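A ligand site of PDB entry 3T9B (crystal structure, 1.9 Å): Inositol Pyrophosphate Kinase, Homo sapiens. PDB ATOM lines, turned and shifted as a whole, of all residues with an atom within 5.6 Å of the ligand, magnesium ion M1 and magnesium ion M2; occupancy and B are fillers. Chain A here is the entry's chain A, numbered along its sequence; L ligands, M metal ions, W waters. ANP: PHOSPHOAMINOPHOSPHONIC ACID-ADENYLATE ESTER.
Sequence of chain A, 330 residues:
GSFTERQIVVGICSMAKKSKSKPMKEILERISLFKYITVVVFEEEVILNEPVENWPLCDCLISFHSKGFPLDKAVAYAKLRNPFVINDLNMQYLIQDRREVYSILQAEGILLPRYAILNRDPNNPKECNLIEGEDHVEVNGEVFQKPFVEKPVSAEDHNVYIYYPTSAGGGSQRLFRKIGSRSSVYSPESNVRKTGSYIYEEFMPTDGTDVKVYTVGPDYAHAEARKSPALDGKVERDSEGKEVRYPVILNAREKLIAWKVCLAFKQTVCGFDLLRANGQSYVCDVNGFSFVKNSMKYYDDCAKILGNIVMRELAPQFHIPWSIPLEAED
Magnesium ion M2 is bound by O1G of the ligand (1.9 Å).
The side-chain carboxylate (OD2) of Asp 273 binds magnesium ion M2.
Magnesium ion M2 is bound by an oxygen (O2A) of the ligand (2.0 Å).
Magnesium ion M2 is bound by water W2.
OD2 of Asp 285 binds magnesium ion M2.
O3G of the ligand is bound to magnesium ion M1, at 1.9 Å.
Magnesium ion M1 is bound by water W1 (2.0 Å).
O2B of the ligand is bound to magnesium ion M1 (2.0 Å).
Magnesium ion M1 is bound by the side-chain amide oxygen (OD1) of Asn 287 (2.1 Å).
Magnesium ion M1 is bound by OD2 of Asp 285 (2.2 Å).
OD1 of Asp 285 binds magnesium ion M1, at 2.3 Å.
Magnesium ion M1 has six donor atoms within binding distance.
Water W2 bridges O3' of the ligand (2.7 Å) and NZ of Lys 212 (3.2 Å).
Water W5 lies within hydrogen-bond range of O2G of the ligand and NE of Arg 177.
Water W7 lies within hydrogen-bond range of O of His 158 (2.7 Å) and O1B of the ligand (2.8 Å).
Water W4 lies within hydrogen-bond range of a nitrogen (N3) of the ligand (2.9 Å) and the side-chain hydroxyl of Ser 228 (3.3 Å).
The backbone carbonyl oxygen (O) of Cys 284 sits close to an oxygen (O1A) of the ligand (3.2 Å).
Merely in contact with the ligand: Pro 113 (3.5 Å), Val 149 (3.7 Å), Val 160 (3.8 Å), Leu 175 (3.4 Å), Phe 203 (3.4 Å), Pro 229 (3.7 Å) and Leu 275 (3.5 Å).
Hydrophobic or aromatic side chains that line the ligand: Pro 113, Val 149, His 158, Val 160, Leu 175, Phe 203, Met 204, Pro 229 and Leu 275.
Within 4 Å of the ligand: Arg 98, Pro 113, Val 149, Lys 151, His 158, Val 160, Leu 175, Arg 177, Glu 201, Glu 202, Phe 203, Met 204, Asp 210, Lys 212, Ser 228, Pro 229, Asp 273, Leu 275, Cys 284, Asp 285 and Asn 287.
Of the 29 residues printed, 2 come within 4 Å of magnesium ion M2.
A nitrogen (N6) of the ligand is in hydrogen-bond range of the backbone carbonyl oxygen (O) of Glu 202, at 2.9 Å.
OE1 of Glu 201 lies within hydrogen-bond range of N6 of the ligand (2.8 Å).
An oxygen (O2') of the ligand lies within hydrogen-bond range of the side-chain hydroxyl of Ser 228.
An oxygen (O1G) of the ligand lies close to the side-chain amino group of Lys 212 (3.97 Å).
The side-chain carboxylate (OD1) of Asp 210 sits at hydrogen-bond distance from an oxygen (O2') of the ligand, at 2.5 Å.
ND1 of His 158 lies within hydrogen-bond range of O1B of the ligand (2.7 Å).
The guanidinium group (NH1) of Arg 177 lies within salt-bridge range of an oxygen (O2G) of the ligand (3.1 Å).
The side-chain amino group (NZ) of Lys 151 lies within salt-bridge range of an oxygen (O1A) of the ligand, 2.8 Å away.
The backbone NH (N) of Met 204 sits at hydrogen-bond distance from a nitrogen (N1) of the ligand (2.8 Å).
NH2 of Arg 98 is in salt-bridge range of O1B of the ligand.
The side-chain hydroxyl of Ser 228 sits at hydrogen-bond distance from the backbone NH of Ala 230 (2.9 Å).
N of Val 149 is in hydrogen-bond range of O of Glu 201, at 2.8 Å.
NE2 of His 158 is in hydrogen-bond range of NH1 of Arg 177 (3.0 Å).
NZ of Lys 212 is in salt-bridge range of OD1 of Asp 273.
The backbone carbonyl oxygen of Val 160 is in hydrogen-bond range of the backbone NH of Leu 175 (2.9 Å).
The backbone carbonyl oxygen (O) of Asp 273 sits at hydrogen-bond distance from the backbone NH (N) of Cys 284 (3.2 Å).
The side-chain hydroxyl of Tyr 102 lies within hydrogen-bond range of the side-chain carboxylate of Glu 201.
O of Cys 284 sits at hydrogen-bond distance from NZ of Lys 151.
The nearest printed residue that does not touch magnesium ion M1 is Arg 98 (4.3 Å).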
ATOM      1  N   ARG A  98     -24.555  10.909 -21.311  1.00  0.00           N
ATOM      2  CA  ARG A  98     -23.687   9.710 -21.220  1.00  0.00           C
ATOM      3  C   ARG A  98     -23.750   8.817 -22.466  1.00  0.00           C
ATOM      4  O   ARG A  98     -22.768   8.155 -22.802  1.00  0.00           O
ATOM      5  CB  ARG A  98     -24.048   8.878 -19.981  1.00  0.00           C
ATOM      6  CG  ARG A  98     -23.765   9.546 -18.632  1.00  0.00           C
ATOM      7  CD  ARG A  98     -23.925   8.515 -17.477  1.00  0.00           C
ATOM      8  NE  ARG A  98     -24.228   9.198 -16.205  1.00  0.00           N
ATOM      9  CZ  ARG A  98     -23.298   9.618 -15.349  1.00  0.00           C
ATOM     10  NH1 ARG A  98     -22.017   9.388 -15.603  1.00  0.00           N
ATOM     11  NH2 ARG A  98     -23.649  10.253 -14.238  1.00  0.00           N
ATOM     12  N   TYR A 102     -20.292   7.829 -24.522  1.00  0.00           N
ATOM     13  CA  TYR A 102     -19.911   6.444 -24.820  1.00  0.00           C
ATOM     14  C   TYR A 102     -19.827   6.176 -26.340  1.00  0.00           C
ATOM     15  O   TYR A 102     -18.957   5.427 -26.795  1.00  0.00           O
ATOM     16  CB  TYR A 102     -20.866   5.495 -24.114  1.00  0.00           C
ATOM     17  CG  TYR A 102     -20.384   5.085 -22.741  1.00  0.00           C
ATOM     18  CD1 TYR A 102     -19.517   5.890 -22.004  1.00  0.00           C
ATOM     19  CD2 TYR A 102     -20.777   3.863 -22.182  1.00  0.00           C
ATOM     20  CE1 TYR A 102     -19.032   5.487 -20.757  1.00  0.00           C
ATOM     21  CE2 TYR A 102     -20.315   3.452 -20.938  1.00  0.00           C
ATOM     22  CZ  TYR A 102     -19.439   4.264 -20.230  1.00  0.00           C
ATOM     23  OH  TYR A 102     -18.982   3.845 -18.990  1.00  0.00           O
ATOM     24  N   PRO A 113     -16.600  -0.158 -20.537  1.00  0.00           N
ATOM     25  CA  PRO A 113     -17.382  -1.302 -20.073  1.00  0.00           C
ATOM     26  C   PRO A 113     -18.425  -1.682 -21.116  1.00  0.00           C
ATOM     27  O   PRO A 113     -18.982  -0.798 -21.766  1.00  0.00           O
ATOM     28  CB  PRO A 113     -18.081  -0.769 -18.804  1.00  0.00           C
ATOM     29  CG  PRO A 113     -17.197   0.375 -18.325  1.00  0.00           C
ATOM     30  CD  PRO A 113     -16.698   0.997 -19.616  1.00  0.00           C
ATOM     31  N   VAL A 149     -23.864  -1.870 -13.250  1.00  0.00           N
ATOM     32  CA  VAL A 149     -23.932  -0.448 -12.923  1.00  0.00           C
ATOM     33  C   VAL A 149     -25.052   0.218 -13.727  1.00  0.00           C
ATOM     34  O   VAL A 149     -25.246  -0.074 -14.914  1.00  0.00           O
ATOM     35  CB  VAL A 149     -22.554   0.244 -13.190  1.00  0.00           C
ATOM     36  CG1 VAL A 149     -22.585   1.705 -12.780  1.00  0.00           C
ATOM     37  CG2 VAL A 149     -21.445  -0.494 -12.442  1.00  0.00           C
ATOM     38  N   LYS A 151     -26.491   3.958 -14.675  1.00  0.00           N
ATOM     39  CA  LYS A 151     -26.189   5.383 -14.719  1.00  0.00           C
ATOM     40  C   LYS A 151     -27.320   6.141 -15.421  1.00  0.00           C
ATOM     41  O   LYS A 151     -27.734   5.763 -16.511  1.00  0.00           O
ATOM     42  CB  LYS A 151     -24.873   5.613 -15.476  1.00  0.00           C
ATOM     43  CG  LYS A 151     -23.676   4.887 -14.884  1.00  0.00           C
ATOM     44  CD  LYS A 151     -22.368   5.244 -15.618  1.00  0.00           C
ATOM     45  CE  LYS A 151     -21.225   4.465 -15.026  1.00  0.00           C
ATOM     46  NZ  LYS A 151     -19.938   4.751 -15.717  1.00  0.00           N
ATOM     47  N   ALA A 155     -25.347  13.006 -17.775  1.00  0.00           N
ATOM     48  CA  ALA A 155     -24.032  12.948 -17.146  1.00  0.00           C
ATOM     49  C   ALA A 155     -23.944  13.864 -15.931  1.00  0.00           C
ATOM     50  O   ALA A 155     -23.041  13.736 -15.111  1.00  0.00           O
ATOM     51  CB  ALA A 155     -22.945  13.287 -18.168  1.00  0.00           C
ATOM     52  N   ASP A 157     -26.355  13.999 -13.673  1.00  0.00           N
ATOM     53  CA  ASP A 157     -27.059  13.297 -12.594  1.00  0.00           C
ATOM     54  C   ASP A 157     -26.119  12.241 -12.031  1.00  0.00           C
ATOM     55  O   ASP A 157     -25.810  11.259 -12.722  1.00  0.00           O
ATOM     56  CB  ASP A 157     -28.338  12.656 -13.155  1.00  0.00           C
ATOM     57  CG  ASP A 157     -29.219  11.999 -12.065  1.00  0.00           C
ATOM     58  OD1 ASP A 157     -28.713  11.660 -10.980  1.00  0.00           O
ATOM     59  OD2 ASP A 157     -30.429  11.826 -12.322  1.00  0.00           O
ATOM     60  N   HIS A 158     -25.665  12.439 -10.794  1.00  0.00           N
ATOM     61  CA  HIS A 158     -24.605  11.590 -10.209  1.00  0.00           C
ATOM     62  C   HIS A 158     -25.147  10.423  -9.375  1.00  0.00           C
ATOM     63  O   HIS A 158     -24.399   9.745  -8.670  1.00  0.00           O
ATOM     64  CB  HIS A 158     -23.603  12.468  -9.444  1.00  0.00           C
ATOM     65  CG  HIS A 158     -22.979  13.520 -10.302  1.00  0.00           C
ATOM     66  ND1 HIS A 158     -22.179  13.208 -11.384  1.00  0.00           N
ATOM     67  CD2 HIS A 158     -23.110  14.872 -10.310  1.00  0.00           C
ATOM     68  CE1 HIS A 158     -21.804  14.329 -11.981  1.00  0.00           C
ATOM     69  NE2 HIS A 158     -22.352  15.344 -11.353  1.00  0.00           N
ATOM     70  N   ASN A 159     -26.438  10.181  -9.507  1.00  0.00           N
ATOM     71  CA  ASN A 159     -27.116   9.103  -8.789  1.00  0.00           C
ATOM     72  C   ASN A 159     -26.943   7.777  -9.553  1.00  0.00           C
ATOM     73  O   ASN A 159     -27.867   7.253 -10.151  1.00  0.00           O
ATOM     74  CB  ASN A 159     -28.582   9.454  -8.561  1.00  0.00           C
ATOM     75  CG  ASN A 159     -28.750  10.675  -7.669  1.00  0.00           C
ATOM     76  OD1 ASN A 159     -28.439  10.628  -6.481  1.00  0.00           O
ATOM     77  ND2 ASN A 159     -29.236  11.778  -8.245  1.00  0.00           N
ATOM     78  N   VAL A 160     -25.706   7.292  -9.515  1.00  0.00           N
ATOM     79  CA  VAL A 160     -25.294   6.061 -10.153  1.00  0.00           C
ATOM     80  C   VAL A 160     -25.480   4.935  -9.146  1.00  0.00           C
ATOM     81  O   VAL A 160     -25.016   5.055  -8.010  1.00  0.00           O
ATOM     82  CB  VAL A 160     -23.802   6.143 -10.571  1.00  0.00           C
ATOM     83  CG1 VAL A 160     -23.275   4.774 -11.014  1.00  0.00           C
ATOM     84  CG2 VAL A 160     -23.656   7.166 -11.689  1.00  0.00           C
ATOM     85  N   ILE A 162     -25.131   0.743  -8.144  1.00  0.00           N
ATOM     86  CA  ILE A 162     -24.509  -0.548  -8.373  1.00  0.00           C
ATOM     87  C   ILE A 162     -25.383  -1.612  -7.716  1.00  0.00           C
ATOM     88  O   ILE A 162     -25.809  -1.449  -6.586  1.00  0.00           O
ATOM     89  CB  ILE A 162     -23.065  -0.547  -7.838  1.00  0.00           C
ATOM     90  CG1 ILE A 162     -22.263   0.547  -8.585  1.00  0.00           C
ATOM     91  CG2 ILE A 162     -22.424  -1.928  -8.047  1.00  0.00           C
ATOM     92  CD1 ILE A 162     -20.943   0.851  -8.022  1.00  0.00           C
ATOM     93  N   LEU A 175     -24.765   5.802  -5.270  1.00  0.00           N
ATOM     94  CA  LEU A 175     -23.714   6.827  -5.291  1.00  0.00           C
ATOM     95  C   LEU A 175     -24.367   8.189  -5.466  1.00  0.00           C
ATOM     96  O   LEU A 175     -25.490   8.283  -5.965  1.00  0.00           O
ATOM     97  CB  LEU A 175     -22.719   6.570  -6.427  1.00  0.00           C
ATOM     98  CG  LEU A 175     -21.662   5.456  -6.276  1.00  0.00           C
ATOM     99  CD1 LEU A 175     -22.247   4.061  -6.088  1.00  0.00           C
ATOM    100  CD2 LEU A 175     -20.756   5.469  -7.504  1.00  0.00           C
ATOM    101  N   ARG A 177     -23.301  12.816  -5.523  1.00  0.00           N
ATOM    102  CA  ARG A 177     -22.321  13.880  -5.353  1.00  0.00           C
ATOM    103  C   ARG A 177     -21.958  13.945  -3.871  1.00  0.00           C
ATOM    104  O   ARG A 177     -22.837  14.038  -3.010  1.00  0.00           O
ATOM    105  CB  ARG A 177     -22.873  15.226  -5.866  1.00  0.00           C
ATOM    106  CG  ARG A 177     -21.839  16.362  -6.034  1.00  0.00           C
ATOM    107  CD  ARG A 177     -20.428  15.886  -6.441  1.00  0.00           C
ATOM    108  NE  ARG A 177     -20.276  15.489  -7.854  1.00  0.00           N
ATOM    109  CZ  ARG A 177     -19.796  16.282  -8.810  1.00  0.00           C
ATOM    110  NH1 ARG A 177     -19.675  15.828 -10.056  1.00  0.00           N
ATOM    111  NH2 ARG A 177     -19.450  17.535  -8.540  1.00  0.00           N
ATOM    112  N   GLU A 201     -24.254  -1.028 -17.404  1.00  0.00           N
ATOM    113  CA  GLU A 201     -22.928  -1.497 -17.781  1.00  0.00           C
ATOM    114  C   GLU A 201     -22.387  -2.586 -16.878  1.00  0.00           C
ATOM    115  O   GLU A 201     -22.700  -2.656 -15.687  1.00  0.00           O
ATOM    116  CB  GLU A 201     -21.917  -0.355 -17.928  1.00  0.00           C
ATOM    117  CG  GLU A 201     -22.029   0.785 -16.981  1.00  0.00           C
ATOM    118  CD  GLU A 201     -21.068   1.922 -17.289  1.00  0.00           C
ATOM    119  OE1 GLU A 201     -19.926   1.858 -16.824  1.00  0.00           O
ATOM    120  OE2 GLU A 201     -21.458   2.917 -17.926  1.00  0.00           O
ATOM    121  N   GLU A 202     -21.526  -3.408 -17.471  1.00  0.00           N
ATOM    122  CA  GLU A 202     -20.825  -4.437 -16.713  1.00  0.00           C
ATOM    123  C   GLU A 202     -19.939  -3.777 -15.652  1.00  0.00           C
ATOM    124  O   GLU A 202     -19.328  -2.722 -15.896  1.00  0.00           O
ATOM    125  CB  GLU A 202     -19.982  -5.305 -17.648  1.00  0.00           C
ATOM    126  CG  GLU A 202     -18.873  -4.565 -18.349  1.00  0.00           C
ATOM    127  CD  GLU A 202     -17.874  -5.484 -19.060  1.00  0.00           C
ATOM    128  OE1 GLU A 202     -17.771  -6.665 -18.676  1.00  0.00           O
ATOM    129  OE2 GLU A 202     -17.207  -5.011 -19.995  1.00  0.00           O
ATOM    130  N   PHE A 203     -19.925  -4.385 -14.480  1.00  0.00           N
ATOM    131  CA  PHE A 203     -19.083  -3.905 -13.393  1.00  0.00           C
ATOM    132  C   PHE A 203     -17.645  -4.350 -13.606  1.00  0.00           C
ATOM    133  O   PHE A 203     -17.376  -5.544 -13.719  1.00  0.00           O
ATOM    134  CB  PHE A 203     -19.604  -4.422 -12.041  1.00  0.00           C
ATOM    135  CG  PHE A 203     -18.841  -3.891 -10.860  1.00  0.00           C
ATOM    136  CD1 PHE A 203     -17.801  -4.635 -10.295  1.00  0.00           C
ATOM    137  CD2 PHE A 203     -19.128  -2.638 -10.346  1.00  0.00           C
ATOM    138  CE1 PHE A 203     -17.082  -4.143  -9.214  1.00  0.00           C
ATOM    139  CE2 PHE A 203     -18.433  -2.134  -9.254  1.00  0.00           C
ATOM    140  CZ  PHE A 203     -17.398  -2.886  -8.693  1.00  0.00           C
ATOM    141  N   MET A 204     -16.732  -3.385 -13.679  1.00  0.00           N
ATOM    142  CA  MET A 204     -15.325  -3.691 -13.883  1.00  0.00           C
ATOM    143  C   MET A 204     -14.615  -3.814 -12.536  1.00  0.00           C
ATOM    144  O   MET A 204     -14.595  -2.843 -11.771  1.00  0.00           O
ATOM    145  CB  MET A 204     -14.639  -2.606 -14.737  1.00  0.00           C
ATOM    146  CG  MET A 204     -15.393  -2.208 -16.008  1.00  0.00           C
ATOM    147  SD  MET A 204     -15.839  -3.588 -17.072  1.00  0.00           S
ATOM    148  CE  MET A 204     -14.226  -4.207 -17.571  1.00  0.00           C
ATOM    149  N   PRO A 205     -14.026  -4.990 -12.240  1.00  0.00           N
ATOM    150  CA  PRO A 205     -13.332  -5.207 -10.976  1.00  0.00           C
ATOM    151  C   PRO A 205     -11.996  -4.474 -10.939  1.00  0.00           C
ATOM    152  O   PRO A 205     -11.141  -4.710 -11.796  1.00  0.00           O
ATOM    153  CB  PRO A 205     -13.108  -6.722 -10.965  1.00  0.00           C
ATOM    154  CG  PRO A 205     -12.999  -7.094 -12.391  1.00  0.00           C
ATOM    155  CD  PRO A 205     -13.903  -6.157 -13.146  1.00  0.00           C
ATOM    156  N   ASP A 210     -10.343   4.454  -8.319  1.00  0.00           N
ATOM    157  CA  ASP A 210     -10.568   5.031  -9.657  1.00  0.00           C
ATOM    158  C   ASP A 210      -9.320   5.819 -10.036  1.00  0.00           C
ATOM    159  O   ASP A 210      -8.740   6.511  -9.185  1.00  0.00           O
ATOM    160  CB  ASP A 210     -11.693   6.064  -9.594  1.00  0.00           C
ATOM    161  CG  ASP A 210     -12.996   5.500  -9.100  1.00  0.00           C
ATOM    162  OD1 ASP A 210     -13.306   4.313  -9.369  1.00  0.00           O
ATOM    163  OD2 ASP A 210     -13.765   6.279  -8.475  1.00  0.00           O
ATOM    164  N   LYS A 212      -8.181   9.041 -11.860  1.00  0.00           N
ATOM    165  CA  LYS A 212      -8.698  10.326 -12.354  1.00  0.00           C
ATOM    166  C   LYS A 212      -7.624  10.950 -13.199  1.00  0.00           C
ATOM    167  O   LYS A 212      -6.499  11.125 -12.736  1.00  0.00           O
ATOM    168  CB  LYS A 212      -8.977  11.293 -11.211  1.00  0.00           C
ATOM    169  CG  LYS A 212      -9.530  10.660  -9.953  1.00  0.00           C
ATOM    170  CD  LYS A 212     -10.946  10.275 -10.121  1.00  0.00           C
ATOM    171  CE  LYS A 212     -11.883  11.471 -10.019  1.00  0.00           C
ATOM    172  NZ  LYS A 212     -13.255  10.904 -10.154  1.00  0.00           N
ATOM    173  N   SER A 228     -12.770   4.209  -4.652  1.00  0.00           N
ATOM    174  CA  SER A 228     -14.032   4.156  -5.406  1.00  0.00           C
ATOM    175  C   SER A 228     -15.212   4.390  -4.467  1.00  0.00           C
ATOM    176  O   SER A 228     -15.286   3.769  -3.407  1.00  0.00           O
ATOM    177  CB  SER A 228     -14.215   2.819  -6.107  1.00  0.00           C
ATOM    178  OG  SER A 228     -15.513   2.765  -6.695  1.00  0.00           O
ATOM    179  N   PRO A 229     -16.147   5.278  -4.856  1.00  0.00           N
ATOM    180  CA  PRO A 229     -17.419   5.398  -4.118  1.00  0.00           C
ATOM    181  C   PRO A 229     -18.270   4.124  -4.241  1.00  0.00           C
ATOM    182  O   PRO A 229     -19.231   3.955  -3.487  1.00  0.00           O
ATOM    183  CB  PRO A 229     -18.126   6.576  -4.791  1.00  0.00           C
ATOM    184  CG  PRO A 229     -17.161   7.184  -5.714  1.00  0.00           C
ATOM    185  CD  PRO A 229     -16.078   6.210  -6.000  1.00  0.00           C
ATOM    186  N   ALA A 230     -17.921   3.256  -5.174  1.00  0.00           N
ATOM    187  CA  ALA A 230     -18.607   1.972  -5.360  1.00  0.00           C
ATOM    188  C   ALA A 230     -18.337   1.001  -4.208  1.00  0.00           C
ATOM    189  O   ALA A 230     -19.041   0.001  -4.078  1.00  0.00           O
ATOM    190  CB  ALA A 230     -18.207   1.346  -6.675  1.00  0.00           C
ATOM    191  N   ASP A 273     -12.281   9.483 -16.172  1.00  0.00           N
ATOM    192  CA  ASP A 273     -11.994   8.440 -15.200  1.00  0.00           C
ATOM    193  C   ASP A 273     -11.623   7.143 -15.911  1.00  0.00           C
ATOM    194  O   ASP A 273     -12.251   6.807 -16.931  1.00  0.00           O
ATOM    195  CB  ASP A 273     -13.220   8.182 -14.329  1.00  0.00           C
ATOM    196  CG  ASP A 273     -13.609   9.373 -13.480  1.00  0.00           C
ATOM    197  OD1 ASP A 273     -12.694  10.051 -12.941  1.00  0.00           O
ATOM    198  OD2 ASP A 273     -14.813   9.628 -13.342  1.00  0.00           O
ATOM    199  N   LEU A 275     -10.841   2.886 -15.186  1.00  0.00           N
ATOM    200  CA  LEU A 275     -10.931   1.738 -14.332  1.00  0.00           C
ATOM    201  C   LEU A 275      -9.858   0.769 -14.777  1.00  0.00           C
ATOM    202  O   LEU A 275      -9.891   0.290 -15.907  1.00  0.00           O
ATOM    203  CB  LEU A 275     -12.312   1.086 -14.442  1.00  0.00           C
ATOM    204  CG  LEU A 275     -13.489   2.031 -14.203  1.00  0.00           C
ATOM    205  CD1 LEU A 275     -14.818   1.311 -14.470  1.00  0.00           C
ATOM    206  CD2 LEU A 275     -13.456   2.661 -12.809  1.00  0.00           C
ATOM    207  N   CYS A 284     -14.780   5.187 -18.004  1.00  0.00           N
ATOM    208  CA  CYS A 284     -16.180   5.026 -17.590  1.00  0.00           C
ATOM    209  C   CYS A 284     -16.930   6.356 -17.497  1.00  0.00           C
ATOM    210  O   CYS A 284     -18.130   6.371 -17.200  1.00  0.00           O
ATOM    211  CB  CYS A 284     -16.266   4.243 -16.262  1.00  0.00           C
ATOM    212  SG  CYS A 284     -15.678   5.181 -14.834  1.00  0.00           S
ATOM    213  N   ASP A 285     -16.232   7.460 -17.779  1.00  0.00           N
ATOM    214  CA  ASP A 285     -16.774   8.798 -17.524  1.00  0.00           C
ATOM    215  C   ASP A 285     -15.869   9.750 -18.271  1.00  0.00           C
ATOM    216  O   ASP A 285     -14.659   9.553 -18.346  1.00  0.00           O
ATOM    217  CB  ASP A 285     -16.848   9.017 -16.000  1.00  0.00           C
ATOM    218  CG  ASP A 285     -17.580  10.293 -15.604  1.00  0.00           C
ATOM    219  OD1 ASP A 285     -18.453  10.814 -16.345  1.00  0.00           O
ATOM    220  OD2 ASP A 285     -17.316  10.767 -14.485  1.00  0.00           O
ATOM    221  N   VAL A 286     -16.456  10.789 -18.864  1.00  0.00           N
ATOM    222  CA  VAL A 286     -15.694  11.917 -19.400  1.00  0.00           C
ATOM    223  C   VAL A 286     -16.378  13.183 -18.893  1.00  0.00           C
ATOM    224  O   VAL A 286     -17.549  13.410 -19.182  1.00  0.00           O
ATOM    225  CB  VAL A 286     -15.637  11.909 -20.950  1.00  0.00           C
ATOM    226  CG1 VAL A 286     -14.918  13.176 -21.461  1.00  0.00           C
ATOM    227  CG2 VAL A 286     -14.943  10.644 -21.474  1.00  0.00           C
ATOM    228  N   ASN A 287     -15.656  13.999 -18.127  1.00  0.00           N
ATOM    229  CA  ASN A 287     -16.250  15.145 -17.452  1.00  0.00           C
ATOM    230  C   ASN A 287     -16.054  16.494 -18.139  1.00  0.00           C
ATOM    231  O   ASN A 287     -16.727  17.462 -17.801  1.00  0.00           O
ATOM    232  CB  ASN A 287     -15.818  15.194 -15.987  1.00  0.00           C
ATOM    233  CG  ASN A 287     -16.363  14.019 -15.214  1.00  0.00           C
ATOM    234  OD1 ASN A 287     -17.509  13.617 -15.427  1.00  0.00           O
ATOM    235  ND2 ASN A 287     -15.552  13.460 -14.302  1.00  0.00           N
HETATM  236  PG  ANP L   1     -18.218  12.233 -11.652  1.00  0.00           P
HETATM  237  O1G ANP L   1     -16.716  11.750 -11.909  1.00  0.00           O
HETATM  238  O2G ANP L   1     -18.274  13.082 -10.410  1.00  0.00           O
HETATM  239  O3G ANP L   1     -18.752  13.044 -12.924  1.00  0.00           O
HETATM  240  PB  ANP L   1     -20.312  10.363 -12.454  1.00  0.00           P
HETATM  241  O1B ANP L   1     -21.652  10.583 -11.848  1.00  0.00           O
HETATM  242  O2B ANP L   1     -20.111  10.849 -13.839  1.00  0.00           O
HETATM  243  N3B ANP L   1     -19.131  10.844 -11.418  1.00  0.00           N
HETATM  244  PA  ANP L   1     -19.111   7.700 -13.034  1.00  0.00           P
HETATM  245  O1A ANP L   1     -19.459   7.162 -14.360  1.00  0.00           O
HETATM  246  O2A ANP L   1     -17.821   8.347 -12.829  1.00  0.00           O
HETATM  247  O3A ANP L   1     -20.268   8.735 -12.487  1.00  0.00           O
HETATM  248  O5' ANP L   1     -19.309   6.588 -11.929  1.00  0.00           O
HETATM  249  C5' ANP L   1     -18.983   6.856 -10.533  1.00  0.00           C
HETATM  250  C4' ANP L   1     -18.068   5.791  -9.915  1.00  0.00           C
HETATM  251  O4' ANP L   1     -18.728   4.510 -10.038  1.00  0.00           O
HETATM  252  C3' ANP L   1     -16.808   5.655 -10.767  1.00  0.00           C
HETATM  253  O3' ANP L   1     -15.822   6.615 -10.337  1.00  0.00           O
HETATM  254  C2' ANP L   1     -16.395   4.227 -10.424  1.00  0.00           C
HETATM  255  O2' ANP L   1     -15.802   4.158  -9.123  1.00  0.00           O
HETATM  256  C1' ANP L   1     -17.755   3.521 -10.346  1.00  0.00           C
HETATM  257  N9  ANP L   1     -18.053   2.930 -11.666  1.00  0.00           N
HETATM  258  C8  ANP L   1     -18.691   3.642 -12.771  1.00  0.00           C
HETATM  259  N7  ANP L   1     -18.894   2.599 -13.744  1.00  0.00           N
HETATM  260  C5  ANP L   1     -18.299   1.482 -13.302  1.00  0.00           C
HETATM  261  C6  ANP L   1     -18.139   0.242 -13.895  1.00  0.00           C
HETATM  262  N6  ANP L   1     -18.624   0.007 -15.118  1.00  0.00           N
HETATM  263  N1  ANP L   1     -17.493  -0.728 -13.205  1.00  0.00           N
HETATM  264  C2  ANP L   1     -17.025  -0.494 -11.981  1.00  0.00           C
HETATM  265  N3  ANP L   1     -17.157   0.685 -11.385  1.00  0.00           N
HETATM  266  C4  ANP L   1     -17.797   1.683 -12.036  1.00  0.00           C
HETATM  267 MG    MG M   1     -18.929  12.253 -14.671  1.00  0.00          MG
HETATM  268 MG    MG M   2     -16.607   9.952 -12.647  1.00  0.00          MG
HETATM  269  O   HOH W   1     -20.376  13.313 -15.439  1.00  0.00           O
HETATM  270  O   HOH W   2     -15.968   9.281 -10.753  1.00  0.00           O
HETATM  271  O   HOH W   3     -14.744  12.892 -10.656  1.00  0.00           O
HETATM  272  O   HOH W   4     -15.530   0.470  -9.043  1.00  0.00           O
HETATM  273  O   HOH W   5     -20.109  12.470  -8.413  1.00  0.00           O
HETATM  274  O   HOH W   6     -18.415  15.711 -13.055  1.00  0.00           O
HETATM  275  O   HOH W   7     -21.881   9.082  -9.484  1.00  0.00           O
